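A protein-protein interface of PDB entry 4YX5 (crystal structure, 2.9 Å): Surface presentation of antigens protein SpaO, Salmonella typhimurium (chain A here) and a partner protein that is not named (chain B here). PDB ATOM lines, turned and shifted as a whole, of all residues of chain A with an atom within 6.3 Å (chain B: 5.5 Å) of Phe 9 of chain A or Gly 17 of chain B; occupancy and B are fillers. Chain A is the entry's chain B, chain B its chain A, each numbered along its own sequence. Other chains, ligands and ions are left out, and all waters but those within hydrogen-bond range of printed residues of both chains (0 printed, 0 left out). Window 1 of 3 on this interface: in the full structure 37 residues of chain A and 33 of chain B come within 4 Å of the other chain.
The backbone NH (N) of Leu 11 of chain A sits at hydrogen-bond distance from the backbone carbonyl oxygen (O) of Phe 14 of chain B, at 2.8 Å. The backbone NH (N) of Ile 16 of chain B sits at hydrogen-bond distance from the backbone carbonyl oxygen (O) of Phe 9 of chain A (2.8 Å). The backbone carbonyl oxygen (O) of Gly 17 of chain B is in hydrogen-bond range of the backbone NH (N) of Phe 9 of chain A (2.7 Å). The backbone carbonyl oxygen of Ser 19 of chain B sits at hydrogen-bond distance from the backbone NH of Leu 7 of chain A (2.7 Å). The backbone carbonyl oxygen (O) of Leu 35 of chain B sits at hydrogen-bond distance from the backbone NH (N) of Val 63 of chain A, 2.9 Å away.
The backbone carbonyl oxygen (O) of Ile 16 of chain B is in hydrogen-bond range of the backbone NH (N) of Arg 41 of chain B. N of Ser 18 of chain B lies within hydrogen-bond range of O of Thr 39 of chain B (2.9 Å). OG of Ser 19 of chain B sits at hydrogen-bond distance from O of Leu 36 of chain B. The backbone carbonyl oxygen (O) of Met 43 of chain A lies within hydrogen-bond range of the backbone NH (N) of Glu 8 of chain A. O of Glu 41 of chain A is in hydrogen-bond range of N of Val 10 of chain A (2.8 Å).
Leu 7 of chain A touches Gly 17 of chain B. Leu 35 of chain B touches Leu 7 of chain A. O of Gly 17 of chain B touches CA of Glu 8 of chain A, 3.5 Å away. Val 15 of chain B touches Phe 9 of chain A. N of Ser 18 of chain B touches CD2 of Phe 9 of chain A, 3.9 Å away. Phe 9 of chain A touches Leu 36 of chain B (CZ to O, 3.9 Å). CD2 of Phe 9 of chain A touches CG1 of Ile 37 of chain B (3.96 Å). Phe 14 of chain B touches Val 10 of chain A. CG2 of Ile 16 of chain B touches CB of Leu 11 of chain A, at 3.6 Å. Gly 62 of chain A touches Leu 35 of chain B.
Of chain B, only Val 15 (3.5 Å), Ile 16 (2.8 Å), Gly 17 (2.7 Å), Ser 18 (3.9 Å), Ser 19 (3.9 Å), Leu 36 (3.9 Å) and Ile 37 (3.96 Å) come within 4 Å of Phe 9 of chain A. Printed residues of chain A within 4 Å of Gly 17 of chain B: Leu 7, Glu 8 and Phe 9. Printed residues of chain B within 4 Å of Leu 7 of chain A: Gly 17 (3.98 Å), Ser 18 (3.2 Å), Ser 19 (2.7 Å) and Leu 35 (3.7 Å). Printed residues of chain B within 4 Å of Leu 11 of chain A: Phe 14 and Ile 16. Arg 41 of chain B touches none of the printed residues of chain A. Glu 41 of chain A touches none of the printed residues of chain B. The nearest residue of chain B that does not touch Phe 9 of chain A is Phe 14 of chain B (4.1 Å).
Printed residues of chain B that touch a printed residue of chain A: Phe 14, Val 15, Ile 16, Gly 17, Ser 18, Ser 19, Leu 35, Leu 36 and Ile 37. Hydrophobic or aromatic side chains of chain B that line the printed part of chain A: Val 15, Ile 16, Leu 35 and Ile 37.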
ATOM      1  N   LEU A   7     -14.257 -18.351   4.100  1.00  0.00           N
ATOM      2  CA  LEU A   7     -14.933 -19.214   5.053  1.00  0.00           C
ATOM      3  C   LEU A   7     -14.168 -19.241   6.346  1.00  0.00           C
ATOM      4  O   LEU A   7     -12.945 -19.381   6.343  1.00  0.00           O
ATOM      5  CB  LEU A   7     -15.065 -20.632   4.522  1.00  0.00           C
ATOM      6  CG  LEU A   7     -16.242 -20.912   3.598  1.00  0.00           C
ATOM      7  CD1 LEU A   7     -16.409 -22.396   3.485  1.00  0.00           C
ATOM      8  CD2 LEU A   7     -17.513 -20.273   4.096  1.00  0.00           C
ATOM      9  N   GLU A   8     -14.895 -19.118   7.449  1.00  0.00           N
ATOM     10  CA  GLU A   8     -14.312 -19.144   8.787  1.00  0.00           C
ATOM     11  C   GLU A   8     -14.792 -20.382   9.520  1.00  0.00           C
ATOM     12  O   GLU A   8     -15.972 -20.727   9.455  1.00  0.00           O
ATOM     13  CB  GLU A   8     -14.706 -17.878   9.555  1.00  0.00           C
ATOM     14  CG  GLU A   8     -13.787 -17.503  10.695  1.00  0.00           C
ATOM     15  CD  GLU A   8     -13.963 -16.043  11.128  1.00  0.00           C
ATOM     16  OE1 GLU A   8     -14.944 -15.746  11.852  1.00  0.00           O
ATOM     17  OE2 GLU A   8     -13.118 -15.191  10.745  1.00  0.00           O
ATOM     18  N   PHE A   9     -13.890 -21.057  10.217  1.00  0.00           N
ATOM     19  CA  PHE A   9     -14.275 -22.226  11.013  1.00  0.00           C
ATOM     20  C   PHE A   9     -14.245 -21.920  12.492  1.00  0.00           C
ATOM     21  O   PHE A   9     -13.175 -21.759  13.079  1.00  0.00           O
ATOM     22  CB  PHE A   9     -13.375 -23.398  10.677  1.00  0.00           C
ATOM     23  CG  PHE A   9     -13.434 -23.752   9.241  1.00  0.00           C
ATOM     24  CD1 PHE A   9     -14.263 -24.749   8.804  1.00  0.00           C
ATOM     25  CD2 PHE A   9     -12.727 -23.026   8.310  1.00  0.00           C
ATOM     26  CE1 PHE A   9     -14.341 -25.055   7.470  1.00  0.00           C
ATOM     27  CE2 PHE A   9     -12.812 -23.322   6.977  1.00  0.00           C
ATOM     28  CZ  PHE A   9     -13.621 -24.337   6.559  1.00  0.00           C
ATOM     29  N   VAL A  10     -15.445 -21.826  13.068  1.00  0.00           N
ATOM     30  CA  VAL A  10     -15.639 -21.360  14.432  1.00  0.00           C
ATOM     31  C   VAL A  10     -15.926 -22.498  15.389  1.00  0.00           C
ATOM     32  O   VAL A  10     -16.998 -23.087  15.368  1.00  0.00           O
ATOM     33  CB  VAL A  10     -16.782 -20.325  14.513  1.00  0.00           C
ATOM     34  CG1 VAL A  10     -16.758 -19.610  15.859  1.00  0.00           C
ATOM     35  CG2 VAL A  10     -16.615 -19.316  13.435  1.00  0.00           C
ATOM     36  N   LEU A  11     -14.950 -22.797  16.233  1.00  0.00           N
ATOM     37  CA  LEU A  11     -15.084 -23.842  17.244  1.00  0.00           C
ATOM     38  C   LEU A  11     -16.132 -23.499  18.301  1.00  0.00           C
ATOM     39  O   LEU A  11     -16.954 -24.336  18.677  1.00  0.00           O
ATOM     40  CB  LEU A  11     -13.741 -24.077  17.915  1.00  0.00           C
ATOM     41  CG  LEU A  11     -13.785 -25.178  18.953  1.00  0.00           C
ATOM     42  CD1 LEU A  11     -14.288 -26.452  18.290  1.00  0.00           C
ATOM     43  CD2 LEU A  11     -12.418 -25.371  19.592  1.00  0.00           C
ATOM     44  N   VAL A  40     -18.749 -27.510  14.874  1.00  0.00           N
ATOM     45  CA  VAL A  40     -17.927 -26.379  14.445  1.00  0.00           C
ATOM     46  C   VAL A  40     -18.733 -25.556  13.478  1.00  0.00           C
ATOM     47  O   VAL A  40     -19.147 -26.052  12.443  1.00  0.00           O
ATOM     48  CB  VAL A  40     -16.628 -26.822  13.744  1.00  0.00           C
ATOM     49  CG1 VAL A  40     -15.903 -25.627  13.112  1.00  0.00           C
ATOM     50  CG2 VAL A  40     -15.724 -27.551  14.702  1.00  0.00           C
ATOM     51  N   GLU A  41     -18.996 -24.309  13.820  1.00  0.00           N
ATOM     52  CA  GLU A  41     -19.802 -23.479  12.936  1.00  0.00           C
ATOM     53  C   GLU A  41     -18.960 -23.025  11.762  1.00  0.00           C
ATOM     54  O   GLU A  41     -17.780 -22.760  11.902  1.00  0.00           O
ATOM     55  CB  GLU A  41     -20.382 -22.271  13.682  1.00  0.00           C
ATOM     56  CG  GLU A  41     -21.689 -22.530  14.432  1.00  0.00           C
ATOM     57  CD  GLU A  41     -21.746 -21.761  15.723  1.00  0.00           C
ATOM     58  OE1 GLU A  41     -20.693 -21.714  16.409  1.00  0.00           O
ATOM     59  OE2 GLU A  41     -22.826 -21.206  16.044  1.00  0.00           O
ATOM     60  N   ILE A  42     -19.579 -22.939  10.598  1.00  0.00           N
ATOM     61  CA  ILE A  42     -18.881 -22.512   9.401  1.00  0.00           C
ATOM     62  C   ILE A  42     -19.437 -21.206   8.938  1.00  0.00           C
ATOM     63  O   ILE A  42     -20.588 -21.129   8.535  1.00  0.00           O
ATOM     64  CB  ILE A  42     -19.023 -23.527   8.288  1.00  0.00           C
ATOM     65  CG1 ILE A  42     -18.376 -24.826   8.716  1.00  0.00           C
ATOM     66  CG2 ILE A  42     -18.376 -23.010   7.005  1.00  0.00           C
ATOM     67  CD1 ILE A  42     -18.579 -25.882   7.741  1.00  0.00           C
ATOM     68  N   MET A  43     -18.619 -20.172   8.983  1.00  0.00           N
ATOM     69  CA  MET A  43     -19.136 -18.847   8.701  1.00  0.00           C
ATOM     70  C   MET A  43     -18.465 -18.211   7.501  1.00  0.00           C
ATOM     71  O   MET A  43     -17.243 -18.138   7.422  1.00  0.00           O
ATOM     72  CB  MET A  43     -18.989 -17.968   9.945  1.00  0.00           C
ATOM     73  CG  MET A  43     -19.910 -18.424  11.070  1.00  0.00           C
ATOM     74  SD  MET A  43     -19.719 -17.446  12.558  1.00  0.00           S
ATOM     75  CE  MET A  43     -19.507 -15.806  11.853  1.00  0.00           C
ATOM     76  N   GLY A  62     -10.479 -30.398   8.391  1.00  0.00           N
ATOM     77  CA  GLY A  62     -11.670 -30.009   7.682  1.00  0.00           C
ATOM     78  C   GLY A  62     -12.880 -30.293   8.519  1.00  0.00           C
ATOM     79  O   GLY A  62     -12.773 -30.851   9.603  1.00  0.00           O
ATOM     80  N   VAL A  63     -14.034 -29.912   7.998  1.00  0.00           N
ATOM     81  CA  VAL A  63     -15.295 -30.062   8.696  1.00  0.00           C
ATOM     82  C   VAL A  63     -16.255 -30.862   7.851  1.00  0.00           C
ATOM     83  O   VAL A  63     -16.682 -30.380   6.813  1.00  0.00           O
ATOM     84  CB  VAL A  63     -15.934 -28.694   9.014  1.00  0.00           C
ATOM     85  CG1 VAL A  63     -17.318 -28.880   9.546  1.00  0.00           C
ATOM     86  CG2 VAL A  63     -15.086 -27.918  10.017  1.00  0.00           C
ATOM     87  N   PHE B  14     -14.197 -18.137  18.642  1.00  0.00           N
ATOM     88  CA  PHE B  14     -12.950 -18.890  18.692  1.00  0.00           C
ATOM     89  C   PHE B  14     -12.695 -19.616  17.373  1.00  0.00           C
ATOM     90  O   PHE B  14     -13.244 -20.681  17.082  1.00  0.00           O
ATOM     91  CB  PHE B  14     -12.979 -19.820  19.876  1.00  0.00           C
ATOM     92  CG  PHE B  14     -13.053 -19.084  21.159  1.00  0.00           C
ATOM     93  CD1 PHE B  14     -11.907 -18.754  21.840  1.00  0.00           C
ATOM     94  CD2 PHE B  14     -14.267 -18.648  21.640  1.00  0.00           C
ATOM     95  CE1 PHE B  14     -11.974 -18.040  22.994  1.00  0.00           C
ATOM     96  CE2 PHE B  14     -14.342 -17.939  22.794  1.00  0.00           C
ATOM     97  CZ  PHE B  14     -13.191 -17.634  23.479  1.00  0.00           C
ATOM     98  N   VAL B  15     -11.865 -18.981  16.566  1.00  0.00           N
ATOM     99  CA  VAL B  15     -11.659 -19.392  15.198  1.00  0.00           C
ATOM    100  C   VAL B  15     -10.508 -20.365  15.119  1.00  0.00           C
ATOM    101  O   VAL B  15      -9.468 -20.112  15.691  1.00  0.00           O
ATOM    102  CB  VAL B  15     -11.386 -18.175  14.312  1.00  0.00           C
ATOM    103  CG1 VAL B  15     -10.853 -18.596  12.973  1.00  0.00           C
ATOM    104  CG2 VAL B  15     -12.647 -17.385  14.154  1.00  0.00           C
ATOM    105  N   ILE B  16     -10.709 -21.489  14.443  1.00  0.00           N
ATOM    106  CA  ILE B  16      -9.650 -22.477  14.286  1.00  0.00           C
ATOM    107  C   ILE B  16      -9.171 -22.514  12.842  1.00  0.00           C
ATOM    108  O   ILE B  16      -8.176 -23.160  12.531  1.00  0.00           O
ATOM    109  CB  ILE B  16     -10.090 -23.905  14.679  1.00  0.00           C
ATOM    110  CG1 ILE B  16     -11.105 -24.460  13.686  1.00  0.00           C
ATOM    111  CG2 ILE B  16     -10.685 -23.938  16.022  1.00  0.00           C
ATOM    112  CD1 ILE B  16     -11.724 -25.735  14.161  1.00  0.00           C
ATOM    113  N   GLY B  17      -9.879 -21.841  11.947  1.00  0.00           N
ATOM    114  CA  GLY B  17      -9.416 -21.820  10.583  1.00  0.00           C
ATOM    115  C   GLY B  17     -10.169 -21.001   9.571  1.00  0.00           C
ATOM    116  O   GLY B  17     -11.305 -20.602   9.763  1.00  0.00           O
ATOM    117  N   SER B  18      -9.504 -20.808   8.447  1.00  0.00           N
ATOM    118  CA  SER B  18      -9.966 -19.978   7.367  1.00  0.00           C
ATOM    119  C   SER B  18      -9.811 -20.747   6.049  1.00  0.00           C
ATOM    120  O   SER B  18      -8.930 -21.595   5.916  1.00  0.00           O
ATOM    121  CB  SER B  18      -9.168 -18.662   7.374  1.00  0.00           C
ATOM    122  OG  SER B  18      -8.947 -18.168   6.061  1.00  0.00           O
ATOM    123  N   SER B  19     -10.679 -20.466   5.083  1.00  0.00           N
ATOM    124  CA  SER B  19     -10.496 -20.971   3.718  1.00  0.00           C
ATOM    125  C   SER B  19     -11.100 -20.033   2.699  1.00  0.00           C
ATOM    126  O   SER B  19     -12.215 -19.583   2.868  1.00  0.00           O
ATOM    127  CB  SER B  19     -11.105 -22.356   3.554  1.00  0.00           C
ATOM    128  OG  SER B  19     -10.157 -23.346   3.885  1.00  0.00           O
ATOM    129  N   LEU B  35     -15.442 -29.724   3.938  1.00  0.00           N
ATOM    130  CA  LEU B  35     -14.765 -28.473   3.616  1.00  0.00           C
ATOM    131  C   LEU B  35     -13.406 -28.434   4.303  1.00  0.00           C
ATOM    132  O   LEU B  35     -13.298 -28.719   5.479  1.00  0.00           O
ATOM    133  CB  LEU B  35     -15.592 -27.272   4.033  1.00  0.00           C
ATOM    134  CG  LEU B  35     -17.045 -27.257   3.575  1.00  0.00           C
ATOM    135  CD1 LEU B  35     -17.665 -25.883   3.793  1.00  0.00           C
ATOM    136  CD2 LEU B  35     -17.104 -27.649   2.135  1.00  0.00           C
ATOM    137  N   LEU B  36     -12.361 -28.106   3.559  1.00  0.00           N
ATOM    138  CA  LEU B  36     -11.019 -28.168   4.106  1.00  0.00           C
ATOM    139  C   LEU B  36     -10.573 -26.826   4.666  1.00  0.00           C
ATOM    140  O   LEU B  36     -10.911 -25.765   4.145  1.00  0.00           O
ATOM    141  CB  LEU B  36     -10.036 -28.642   3.046  1.00  0.00           C
ATOM    142  CG  LEU B  36      -9.980 -30.094   2.562  1.00  0.00           C
ATOM    143  CD1 LEU B  36      -8.842 -30.205   1.549  1.00  0.00           C
ATOM    144  CD2 LEU B  36      -9.795 -31.116   3.690  1.00  0.00           C
ATOM    145  N   ILE B  37      -9.815 -26.886   5.747  1.00  0.00           N
ATOM    146  CA  ILE B  37      -9.244 -25.700   6.354  1.00  0.00           C
ATOM    147  C   ILE B  37      -7.867 -25.462   5.739  1.00  0.00           C
ATOM    148  O   ILE B  37      -6.894 -26.128   6.098  1.00  0.00           O
ATOM    149  CB  ILE B  37      -9.110 -25.847   7.894  1.00  0.00           C
ATOM    150  CG1 ILE B  37     -10.438 -26.249   8.516  1.00  0.00           C
ATOM    151  CG2 ILE B  37      -8.633 -24.554   8.524  1.00  0.00           C
ATOM    152  CD1 ILE B  37     -10.265 -26.900   9.827  1.00  0.00           C
ATOM    153  N   THR B  39      -6.142 -22.452   5.764  1.00  0.00           N
ATOM    154  CA  THR B  39      -5.349 -21.655   6.707  1.00  0.00           C
ATOM    155  C   THR B  39      -5.688 -22.020   8.162  1.00  0.00           C
ATOM    156  O   THR B  39      -6.826 -21.923   8.589  1.00  0.00           O
ATOM    157  CB  THR B  39      -5.577 -20.149   6.494  1.00  0.00           C
ATOM    158  OG1 THR B  39      -5.181 -19.786   5.169  1.00  0.00           O
ATOM    159  CG2 THR B  39      -4.768 -19.359   7.469  1.00  0.00           C
ATOM    160  N   SER B  40      -4.702 -22.435   8.935  1.00  0.00           N
ATOM    161  CA  SER B  40      -5.007 -22.932  10.255  1.00  0.00           C
ATOM    162  C   SER B  40      -4.575 -21.967  11.347  1.00  0.00           C
ATOM    163  O   SER B  40      -3.426 -21.540  11.386  1.00  0.00           O
ATOM    164  CB  SER B  40      -4.356 -24.281  10.479  1.00  0.00           C
ATOM    165  OG  SER B  40      -4.567 -24.679  11.817  1.00  0.00           O
ATOM    166  N   ARG B  41      -5.516 -21.651  12.240  1.00  0.00           N
ATOM    167  CA  ARG B  41      -5.365 -20.607  13.246  1.00  0.00           C
ATOM    168  C   ARG B  41      -5.810 -21.124  14.599  1.00  0.00           C
ATOM    169  O   ARG B  41      -6.343 -22.218  14.694  1.00  0.00           O
ATOM    170  CB  ARG B  41      -6.196 -19.362  12.872  1.00  0.00           C
ATOM    171  CG  ARG B  41      -6.101 -18.912  11.411  1.00  0.00           C
ATOM    172  CD  ARG B  41      -6.986 -17.706  11.105  1.00  0.00           C
ATOM    173  NE  ARG B  41      -7.028 -17.415   9.675  1.00  0.00           N
ATOM    174  CZ  ARG B  41      -6.418 -16.393   9.091  1.00  0.00           C
ATOM    175  NH1 ARG B  41      -5.737 -15.513   9.809  1.00  0.00           N
ATOM    176  NH2 ARG B  41      -6.511 -16.238   7.776  1.00  0.00           N
